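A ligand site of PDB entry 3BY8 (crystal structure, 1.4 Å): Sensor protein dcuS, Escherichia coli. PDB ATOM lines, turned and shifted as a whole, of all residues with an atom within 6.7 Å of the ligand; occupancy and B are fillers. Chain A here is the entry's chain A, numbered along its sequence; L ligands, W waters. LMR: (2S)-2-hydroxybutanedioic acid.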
ATOM      1  N   LEU A  57     -18.740   0.630 -30.371  1.00  0.00           N
ATOM      2  CA  LEU A  57     -19.917   0.228 -29.621  1.00  0.00           C
ATOM      3  C   LEU A  57     -20.747   1.402 -29.108  1.00  0.00           C
ATOM      4  O   LEU A  57     -21.956   1.369 -29.074  1.00  0.00           O
ATOM      5  CB  LEU A  57     -19.489  -0.651 -28.430  1.00  0.00           C
ATOM      6  CG  LEU A  57     -20.635  -1.122 -27.517  1.00  0.00           C
ATOM      7  CD1 LEU A  57     -21.459  -2.219 -28.215  1.00  0.00           C
ATOM      8  CD2 LEU A  57     -20.048  -1.694 -26.209  1.00  0.00           C
ATOM      9  N   PHE A  58     -20.052   2.433 -28.627  1.00  0.00           N
ATOM     10  CA  PHE A  58     -20.776   3.589 -28.144  1.00  0.00           C
ATOM     11  C   PHE A  58     -19.889   4.836 -28.097  1.00  0.00           C
ATOM     12  O   PHE A  58     -18.685   4.739 -27.989  1.00  0.00           O
ATOM     13  CB  PHE A  58     -21.302   3.348 -26.705  1.00  0.00           C
ATOM     14  CG  PHE A  58     -20.212   3.323 -25.625  1.00  0.00           C
ATOM     15  CD1 PHE A  58     -19.695   4.518 -25.088  1.00  0.00           C
ATOM     16  CD2 PHE A  58     -19.785   2.113 -25.081  1.00  0.00           C
ATOM     17  CE1 PHE A  58     -18.763   4.475 -24.030  1.00  0.00           C
ATOM     18  CE2 PHE A  58     -18.858   2.072 -24.014  1.00  0.00           C
ATOM     19  CZ  PHE A  58     -18.343   3.257 -23.488  1.00  0.00           C
ATOM     20  N   VAL A  60     -20.331   8.233 -25.917  1.00  0.00           N
ATOM     21  CA  VAL A  60     -21.089   8.925 -24.902  1.00  0.00           C
ATOM     22  C   VAL A  60     -20.374  10.199 -24.418  1.00  0.00           C
ATOM     23  O   VAL A  60     -19.301  10.138 -23.829  1.00  0.00           O
ATOM     24  CB  VAL A  60     -21.293   7.962 -23.696  1.00  0.00           C
ATOM     25  CG1 VAL A  60     -21.842   8.710 -22.476  1.00  0.00           C
ATOM     26  CG2 VAL A  60     -22.240   6.846 -24.116  1.00  0.00           C
ATOM     27  N   ARG A  68     -25.110  12.167 -19.282  1.00  0.00           N
ATOM     28  CA  ARG A  68     -24.945  11.855 -20.690  1.00  0.00           C
ATOM     29  C   ARG A  68     -25.646  12.761 -21.682  1.00  0.00           C
ATOM     30  O   ARG A  68     -26.817  13.120 -21.461  1.00  0.00           O
ATOM     31  CB  ARG A  68     -25.442  10.438 -20.985  1.00  0.00           C
ATOM     32  CG  ARG A  68     -24.849   9.325 -20.145  1.00  0.00           C
ATOM     33  CD  ARG A  68     -25.247   8.031 -20.806  1.00  0.00           C
ATOM     34  NE  ARG A  68     -24.970   6.847 -19.994  1.00  0.00           N
ATOM     35  CZ  ARG A  68     -25.740   6.428 -18.986  1.00  0.00           C
ATOM     36  NH1 ARG A  68     -26.829   7.113 -18.626  1.00  0.00           N
ATOM     37  NH2 ARG A  68     -25.457   5.294 -18.360  1.00  0.00           N
ATOM     38  N   SER A  70     -25.291  11.765 -25.018  1.00  0.00           N
ATOM     39  CA  SER A  70     -25.479  10.813 -26.103  1.00  0.00           C
ATOM     40  C   SER A  70     -25.311   9.405 -25.557  1.00  0.00           C
ATOM     41  O   SER A  70     -24.666   9.210 -24.505  1.00  0.00           O
ATOM     42  CB  SER A  70     -24.470  11.044 -27.219  1.00  0.00           C
ATOM     43  OG  SER A  70     -23.126  10.889 -26.780  1.00  0.00           O
ATOM     44  N   HIS A  71     -25.917   8.441 -26.243  1.00  0.00           N
ATOM     45  CA  HIS A  71     -25.828   7.014 -25.903  1.00  0.00           C
ATOM     46  C   HIS A  71     -26.577   6.243 -26.973  1.00  0.00           C
ATOM     47  O   HIS A  71     -27.550   6.762 -27.499  1.00  0.00           O
ATOM     48  CB  HIS A  71     -26.516   6.732 -24.564  1.00  0.00           C
ATOM     49  CG  HIS A  71     -26.188   5.382 -23.986  1.00  0.00           C
ATOM     50  ND1 HIS A  71     -26.817   4.214 -24.366  1.00  0.00           N
ATOM     51  CD2 HIS A  71     -25.296   5.033 -23.027  1.00  0.00           C
ATOM     52  CE1 HIS A  71     -26.330   3.202 -23.671  1.00  0.00           C
ATOM     53  NE2 HIS A  71     -25.407   3.679 -22.852  1.00  0.00           N
ATOM     54  N   PRO A  72     -26.136   5.018 -27.310  1.00  0.00           N
ATOM     55  CA  PRO A  72     -26.877   4.274 -28.337  1.00  0.00           C
ATOM     56  C   PRO A  72     -28.340   4.082 -27.962  1.00  0.00           C
ATOM     57  O   PRO A  72     -29.198   3.964 -28.845  1.00  0.00           O
ATOM     58  CB  PRO A  72     -26.126   2.959 -28.430  1.00  0.00           C
ATOM     59  CG  PRO A  72     -24.718   3.361 -28.143  1.00  0.00           C
ATOM     60  CD  PRO A  72     -24.861   4.343 -27.003  1.00  0.00           C
ATOM     61  N   GLU A  73     -28.623   4.010 -26.655  1.00  0.00           N
ATOM     62  CA  GLU A  73     -29.978   3.888 -26.113  1.00  0.00           C
ATOM     63  C   GLU A  73     -30.373   5.300 -25.700  1.00  0.00           C
ATOM     64  O   GLU A  73     -29.967   5.802 -24.636  1.00  0.00           O
ATOM     65  CB  GLU A  73     -30.003   2.942 -24.908  1.00  0.00           C
ATOM     66  CG  GLU A  73     -29.535   1.543 -25.262  1.00  0.00           C
ATOM     67  CD  GLU A  73     -29.507   0.601 -24.065  1.00  0.00           C
ATOM     68  OE1 GLU A  73     -29.816   1.051 -22.924  1.00  0.00           O
ATOM     69  OE2 GLU A  73     -29.177  -0.575 -24.291  1.00  0.00           O
ATOM     70  N   ARG A  76     -31.138   6.865 -22.218  1.00  0.00           N
ATOM     71  CA  ARG A  76     -30.125   7.097 -21.194  1.00  0.00           C
ATOM     72  C   ARG A  76     -29.533   8.490 -21.186  1.00  0.00           C
ATOM     73  O   ARG A  76     -28.723   8.844 -20.335  1.00  0.00           O
ATOM     74  CB  ARG A  76     -29.048   6.032 -21.308  1.00  0.00           C
ATOM     75  CG  ARG A  76     -29.660   4.656 -21.092  1.00  0.00           C
ATOM     76  CD  ARG A  76     -28.665   3.571 -20.857  1.00  0.00           C
ATOM     77  NE  ARG A  76     -29.340   2.288 -20.688  1.00  0.00           N
ATOM     78  CZ  ARG A  76     -29.997   1.906 -19.594  1.00  0.00           C
ATOM     79  NH1 ARG A  76     -30.085   2.701 -18.532  1.00  0.00           N
ATOM     80  NH2 ARG A  76     -30.569   0.707 -19.567  1.00  0.00           N
ATOM     81  N   PRO A  80     -26.859   9.758 -15.288  1.00  0.00           N
ATOM     82  CA  PRO A  80     -25.426   9.617 -15.009  1.00  0.00           C
ATOM     83  C   PRO A  80     -24.763   8.436 -15.686  1.00  0.00           C
ATOM     84  O   PRO A  80     -25.311   7.325 -15.777  1.00  0.00           O
ATOM     85  CB  PRO A  80     -25.361   9.454 -13.498  1.00  0.00           C
ATOM     86  CG  PRO A  80     -26.681   9.970 -12.997  1.00  0.00           C
ATOM     87  CD  PRO A  80     -27.647   9.563 -14.061  1.00  0.00           C
ATOM     88  N   PHE A  81     -23.542   8.698 -16.152  1.00  0.00           N
ATOM     89  CA  PHE A  81     -22.710   7.676 -16.758  1.00  0.00           C
ATOM     90  C   PHE A  81     -22.524   6.495 -15.782  1.00  0.00           C
ATOM     91  O   PHE A  81     -22.434   6.710 -14.568  1.00  0.00           O
ATOM     92  CB  PHE A  81     -21.353   8.291 -17.064  1.00  0.00           C
ATOM     93  CG  PHE A  81     -20.431   7.389 -17.847  1.00  0.00           C
ATOM     94  CD1 PHE A  81     -19.546   6.527 -17.216  1.00  0.00           C
ATOM     95  CD2 PHE A  81     -20.482   7.381 -19.250  1.00  0.00           C
ATOM     96  CE1 PHE A  81     -18.727   5.676 -17.930  1.00  0.00           C
ATOM     97  CE2 PHE A  81     -19.667   6.523 -19.988  1.00  0.00           C
ATOM     98  CZ  PHE A  81     -18.791   5.671 -19.354  1.00  0.00           C
ATOM     99  N   LYS A  82     -22.485   5.279 -16.299  1.00  0.00           N
ATOM    100  CA  LYS A  82     -22.251   4.108 -15.469  1.00  0.00           C
ATOM    101  C   LYS A  82     -20.860   3.557 -15.747  1.00  0.00           C
ATOM    102  O   LYS A  82     -20.563   3.160 -16.867  1.00  0.00           O
ATOM    103  CB  LYS A  82     -23.302   3.025 -15.731  1.00  0.00           C
ATOM    104  CG  LYS A  82     -23.027   1.777 -14.885  1.00  0.00           C
ATOM    105  CD  LYS A  82     -23.956   0.620 -15.207  1.00  0.00           C
ATOM    106  CE  LYS A  82     -25.281   0.757 -14.504  1.00  0.00           C
ATOM    107  NZ  LYS A  82     -26.097  -0.483 -14.720  1.00  0.00           N
ATOM    108  N   GLY A  83     -20.005   3.559 -14.725  1.00  0.00           N
ATOM    109  CA  GLY A  83     -18.652   3.062 -14.864  1.00  0.00           C
ATOM    110  C   GLY A  83     -17.671   3.975 -14.153  1.00  0.00           C
ATOM    111  O   GLY A  83     -17.634   5.196 -14.440  1.00  0.00           O
ATOM    112  N   ASP A  85     -14.641   4.101 -14.579  1.00  0.00           N
ATOM    113  CA  ASP A  85     -13.541   4.463 -15.453  1.00  0.00           C
ATOM    114  C   ASP A  85     -13.606   5.870 -16.024  1.00  0.00           C
ATOM    115  O   ASP A  85     -12.597   6.366 -16.517  1.00  0.00           O
ATOM    116  CB  ASP A  85     -13.281   3.388 -16.541  1.00  0.00           C
ATOM    117  CG  ASP A  85     -14.560   2.827 -17.202  1.00  0.00           C
ATOM    118  OD1 ASP A  85     -15.684   2.876 -16.667  1.00  0.00           O
ATOM    119  OD2 ASP A  85     -14.384   2.275 -18.307  1.00  0.00           O
ATOM    120  N   ASN A  99     -14.706  -2.454 -19.056  1.00  0.00           N
ATOM    121  CA  ASN A  99     -15.839  -2.335 -18.130  1.00  0.00           C
ATOM    122  C   ASN A  99     -17.139  -2.404 -18.905  1.00  0.00           C
ATOM    123  O   ASN A  99     -17.152  -2.718 -20.110  1.00  0.00           O
ATOM    124  CB  ASN A  99     -15.741  -0.973 -17.397  1.00  0.00           C
ATOM    125  CG  ASN A  99     -16.478  -0.935 -16.061  1.00  0.00           C
ATOM    126  OD1 ASN A  99     -17.003  -1.940 -15.599  1.00  0.00           O
ATOM    127  ND2 ASN A  99     -16.512   0.239 -15.452  1.00  0.00           N
ATOM    128  N   ARG A 100     -18.240  -2.134 -18.213  1.00  0.00           N
ATOM    129  CA  ARG A 100     -19.522  -2.078 -18.905  1.00  0.00           C
ATOM    130  C   ARG A 100     -20.490  -1.250 -18.096  1.00  0.00           C
ATOM    131  O   ARG A 100     -20.359  -1.138 -16.881  1.00  0.00           O
ATOM    132  CB  ARG A 100     -20.109  -3.471 -19.139  1.00  0.00           C
ATOM    133  CG  ARG A 100     -20.496  -4.214 -17.914  1.00  0.00           C
ATOM    134  CD  ARG A 100     -21.387  -5.392 -18.316  1.00  0.00           C
ATOM    135  NE  ARG A 100     -22.728  -4.883 -18.561  1.00  0.00           N
ATOM    136  CZ  ARG A 100     -23.649  -5.484 -19.297  1.00  0.00           C
ATOM    137  NH1 ARG A 100     -23.389  -6.656 -19.877  1.00  0.00           N
ATOM    138  NH2 ARG A 100     -24.828  -4.900 -19.456  1.00  0.00           N
ATOM    139  N   GLY A 101     -21.392  -0.601 -18.825  1.00  0.00           N
ATOM    140  CA  GLY A 101     -22.452   0.178 -18.230  1.00  0.00           C
ATOM    141  C   GLY A 101     -23.709  -0.642 -18.491  1.00  0.00           C
ATOM    142  O   GLY A 101     -23.927  -1.661 -17.838  1.00  0.00           O
ATOM    143  N   PHE A 102     -24.515  -0.231 -19.474  1.00  0.00           N
ATOM    144  CA  PHE A 102     -25.714  -0.968 -19.854  1.00  0.00           C
ATOM    145  C   PHE A 102     -25.540  -1.774 -21.141  1.00  0.00           C
ATOM    146  O   PHE A 102     -26.364  -2.643 -21.466  1.00  0.00           O
ATOM    147  CB  PHE A 102     -26.901  -0.014 -19.977  1.00  0.00           C
ATOM    148  CG  PHE A 102     -27.277   0.576 -18.673  1.00  0.00           C
ATOM    149  CD1 PHE A 102     -28.015  -0.182 -17.760  1.00  0.00           C
ATOM    150  CD2 PHE A 102     -26.826   1.831 -18.294  1.00  0.00           C
ATOM    151  CE1 PHE A 102     -28.272   0.301 -16.480  1.00  0.00           C
ATOM    152  CE2 PHE A 102     -27.081   2.327 -17.018  1.00  0.00           C
ATOM    153  CZ  PHE A 102     -27.809   1.560 -16.108  1.00  0.00           C
ATOM    154  N   LEU A 103     -24.489  -1.474 -21.898  1.00  0.00           N
ATOM    155  CA  LEU A 103     -24.221  -2.167 -23.151  1.00  0.00           C
ATOM    156  C   LEU A 103     -23.299  -3.343 -22.887  1.00  0.00           C
ATOM    157  O   LEU A 103     -23.041  -3.681 -21.719  1.00  0.00           O
ATOM    158  CB  LEU A 103     -23.581  -1.196 -24.152  1.00  0.00           C
ATOM    159  CG  LEU A 103     -24.437   0.054 -24.407  1.00  0.00           C
ATOM    160  CD1 LEU A 103     -23.680   1.015 -25.327  1.00  0.00           C
ATOM    161  CD2 LEU A 103     -25.787  -0.335 -25.029  1.00  0.00           C
ATOM    162  N   ALA A 104     -22.787  -3.984 -23.939  1.00  0.00           N
ATOM    163  CA  ALA A 104     -21.900  -5.120 -23.757  1.00  0.00           C
ATOM    164  C   ALA A 104     -20.586  -4.681 -23.114  1.00  0.00           C
ATOM    165  O   ALA A 104     -20.228  -3.482 -23.104  1.00  0.00           O
ATOM    166  CB  ALA A 104     -21.606  -5.761 -25.101  1.00  0.00           C
ATOM    167  N   GLN A 105     -19.861  -5.648 -22.570  1.00  0.00           N
ATOM    168  CA  GLN A 105     -18.548  -5.448 -21.981  1.00  0.00           C
ATOM    169  C   GLN A 105     -17.674  -4.896 -23.090  1.00  0.00           C
ATOM    170  O   GLN A 105     -17.733  -5.348 -24.256  1.00  0.00           O
ATOM    171  CB  GLN A 105     -18.016  -6.777 -21.479  1.00  0.00           C
ATOM    172  CG  GLN A 105     -18.803  -7.276 -20.293  1.00  0.00           C
ATOM    173  CD  GLN A 105     -18.257  -8.564 -19.774  1.00  0.00           C
ATOM    174  OE1 GLN A 105     -18.608  -9.022 -18.673  1.00  0.00           O
ATOM    175  NE2 GLN A 105     -17.364  -9.170 -20.553  1.00  0.00           N
ATOM    176  N   ALA A 106     -16.845  -3.925 -22.717  1.00  0.00           N
ATOM    177  CA  ALA A 106     -16.065  -3.200 -23.691  1.00  0.00           C
ATOM    178  C   ALA A 106     -14.732  -2.665 -23.243  1.00  0.00           C
ATOM    179  O   ALA A 106     -14.479  -2.514 -22.059  1.00  0.00           O
ATOM    180  CB  ALA A 106     -16.919  -2.010 -24.151  1.00  0.00           C
ATOM    181  N   ARG A 108     -12.842   0.529 -23.265  1.00  0.00           N
ATOM    182  CA  ARG A 108     -13.346   1.904 -23.237  1.00  0.00           C
ATOM    183  C   ARG A 108     -12.260   2.922 -23.051  1.00  0.00           C
ATOM    184  O   ARG A 108     -11.327   2.723 -22.296  1.00  0.00           O
ATOM    185  CB  ARG A 108     -14.350   1.983 -22.079  1.00  0.00           C
ATOM    186  CG  ARG A 108     -15.514   1.017 -22.256  1.00  0.00           C
ATOM    187  CD  ARG A 108     -16.006   0.365 -20.930  1.00  0.00           C
ATOM    188  NE  ARG A 108     -16.403   1.315 -19.884  1.00  0.00           N
ATOM    189  CZ  ARG A 108     -17.650   1.655 -19.614  1.00  0.00           C
ATOM    190  NH1 ARG A 108     -18.681   1.175 -20.299  1.00  0.00           N
ATOM    191  NH2 ARG A 108     -17.885   2.461 -18.566  1.00  0.00           N
ATOM    192  N   ALA A 125     -16.511   9.670 -23.946  1.00  0.00           N
ATOM    193  CA  ALA A 125     -16.265   8.269 -23.612  1.00  0.00           C
ATOM    194  C   ALA A 125     -16.620   7.406 -24.836  1.00  0.00           C
ATOM    195  O   ALA A 125     -17.708   7.567 -25.399  1.00  0.00           O
ATOM    196  CB  ALA A 125     -17.153   7.862 -22.422  1.00  0.00           C
HETATM  197  C1  LMR L   1     -22.446   4.531 -20.101  1.00  0.00           C
HETATM  198  O1A LMR L   1     -22.979   5.198 -20.956  1.00  0.00           O
HETATM  199  O1B LMR L   1     -22.950   4.451 -18.964  1.00  0.00           O
HETATM  200  C2  LMR L   1     -21.428   3.529 -20.562  1.00  0.00           C
HETATM  201  O2  LMR L   1     -21.031   2.610 -19.446  1.00  0.00           O
HETATM  202  C3  LMR L   1     -21.815   2.824 -21.876  1.00  0.00           C
HETATM  203  C4  LMR L   1     -22.764   1.655 -21.565  1.00  0.00           C
HETATM  204  O4A LMR L   1     -23.930   1.896 -21.236  1.00  0.00           O
HETATM  205  O4B LMR L   1     -22.326   0.469 -21.593  1.00  0.00           O
HETATM  206  O   HOH W   1     -19.914  -0.756 -22.153  1.00  0.00           O
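CE2 of Phe 58 touches C3 of the ligand (3.7 Å).
Val 60 touches the ligand.
CE2 of Phe 81 touches C1 of the ligand, 3.4 Å away.
Ten residues have an atom within 4 Å of the ligand: Phe 58, Val 60, Arg 68, His 71, Phe 81, Lys 82, Gly 101, Phe 102, Leu 103 and Arg 108.
The nearest printed residue that does not touch the ligand is Arg 100 (4.1 Å).
The guanidinium group (NH2) of Arg 108 is in hydrogen-bond range of the backbone carbonyl oxygen (O) of Lys 82, 3.2 Å away.
O of Pro 80 sits at hydrogen-bond distance from NH1 of Arg 68 (3.2 Å).
The backbone carbonyl oxygen (O) of Arg 76 lies within hydrogen-bond range of the guanidinium group (NH1) of Arg 68, at 3.1 Å.
O of Phe 102 sits at hydrogen-bond distance from NH2 of Arg 100 (3.4 Å).
A ring nitrogen (ND1) of His 71 sits at hydrogen-bond distance from the backbone NH of Glu 73 (2.9 Å).
NE of Arg 108 is in salt-bridge range of OD2 of Asp 85 (2.7 Å).
The backbone carbonyl oxygen (O) of Leu 103 lies close to the guanidinium group (NH2) of Arg 100 (3.1 Å).
The backbone carbonyl oxygen of Ala 125 lies within hydrogen-bond range of the backbone NH of Val 60 (2.8 Å).
Water W1 lies within hydrogen-bond range of an oxygen (O4B) of the ligand, the backbone carbonyl oxygen (O) of Ala 104 and the guanidinium group (NH1) of Arg 108.
An oxygen (O1B) of the ligand sits at hydrogen-bond distance from the backbone NH (N) of Lys 82, at 2.8 Å.
O of Lys 82 sits at hydrogen-bond distance from O2 of the ligand, at 2.7 Å.
NH2 of Arg 68 lies within salt-bridge range of O1B of the ligand, 2.7 Å away.
N of Phe 102 is in hydrogen-bond range of O4A of the ligand, at 2.8 Å.
NE2 of His 71 lies within hydrogen-bond range of O4A of the ligand (2.8 Å).
O4B of the ligand is in salt-bridge range of NH1 of Arg 108 (3.9 Å).
An oxygen (O4B) of the ligand is in hydrogen-bond range of the backbone NH (N) of Leu 103, 2.9 Å away.
N of Gly 101 sits at hydrogen-bond distance from O4B of the ligand (3.1 Å).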
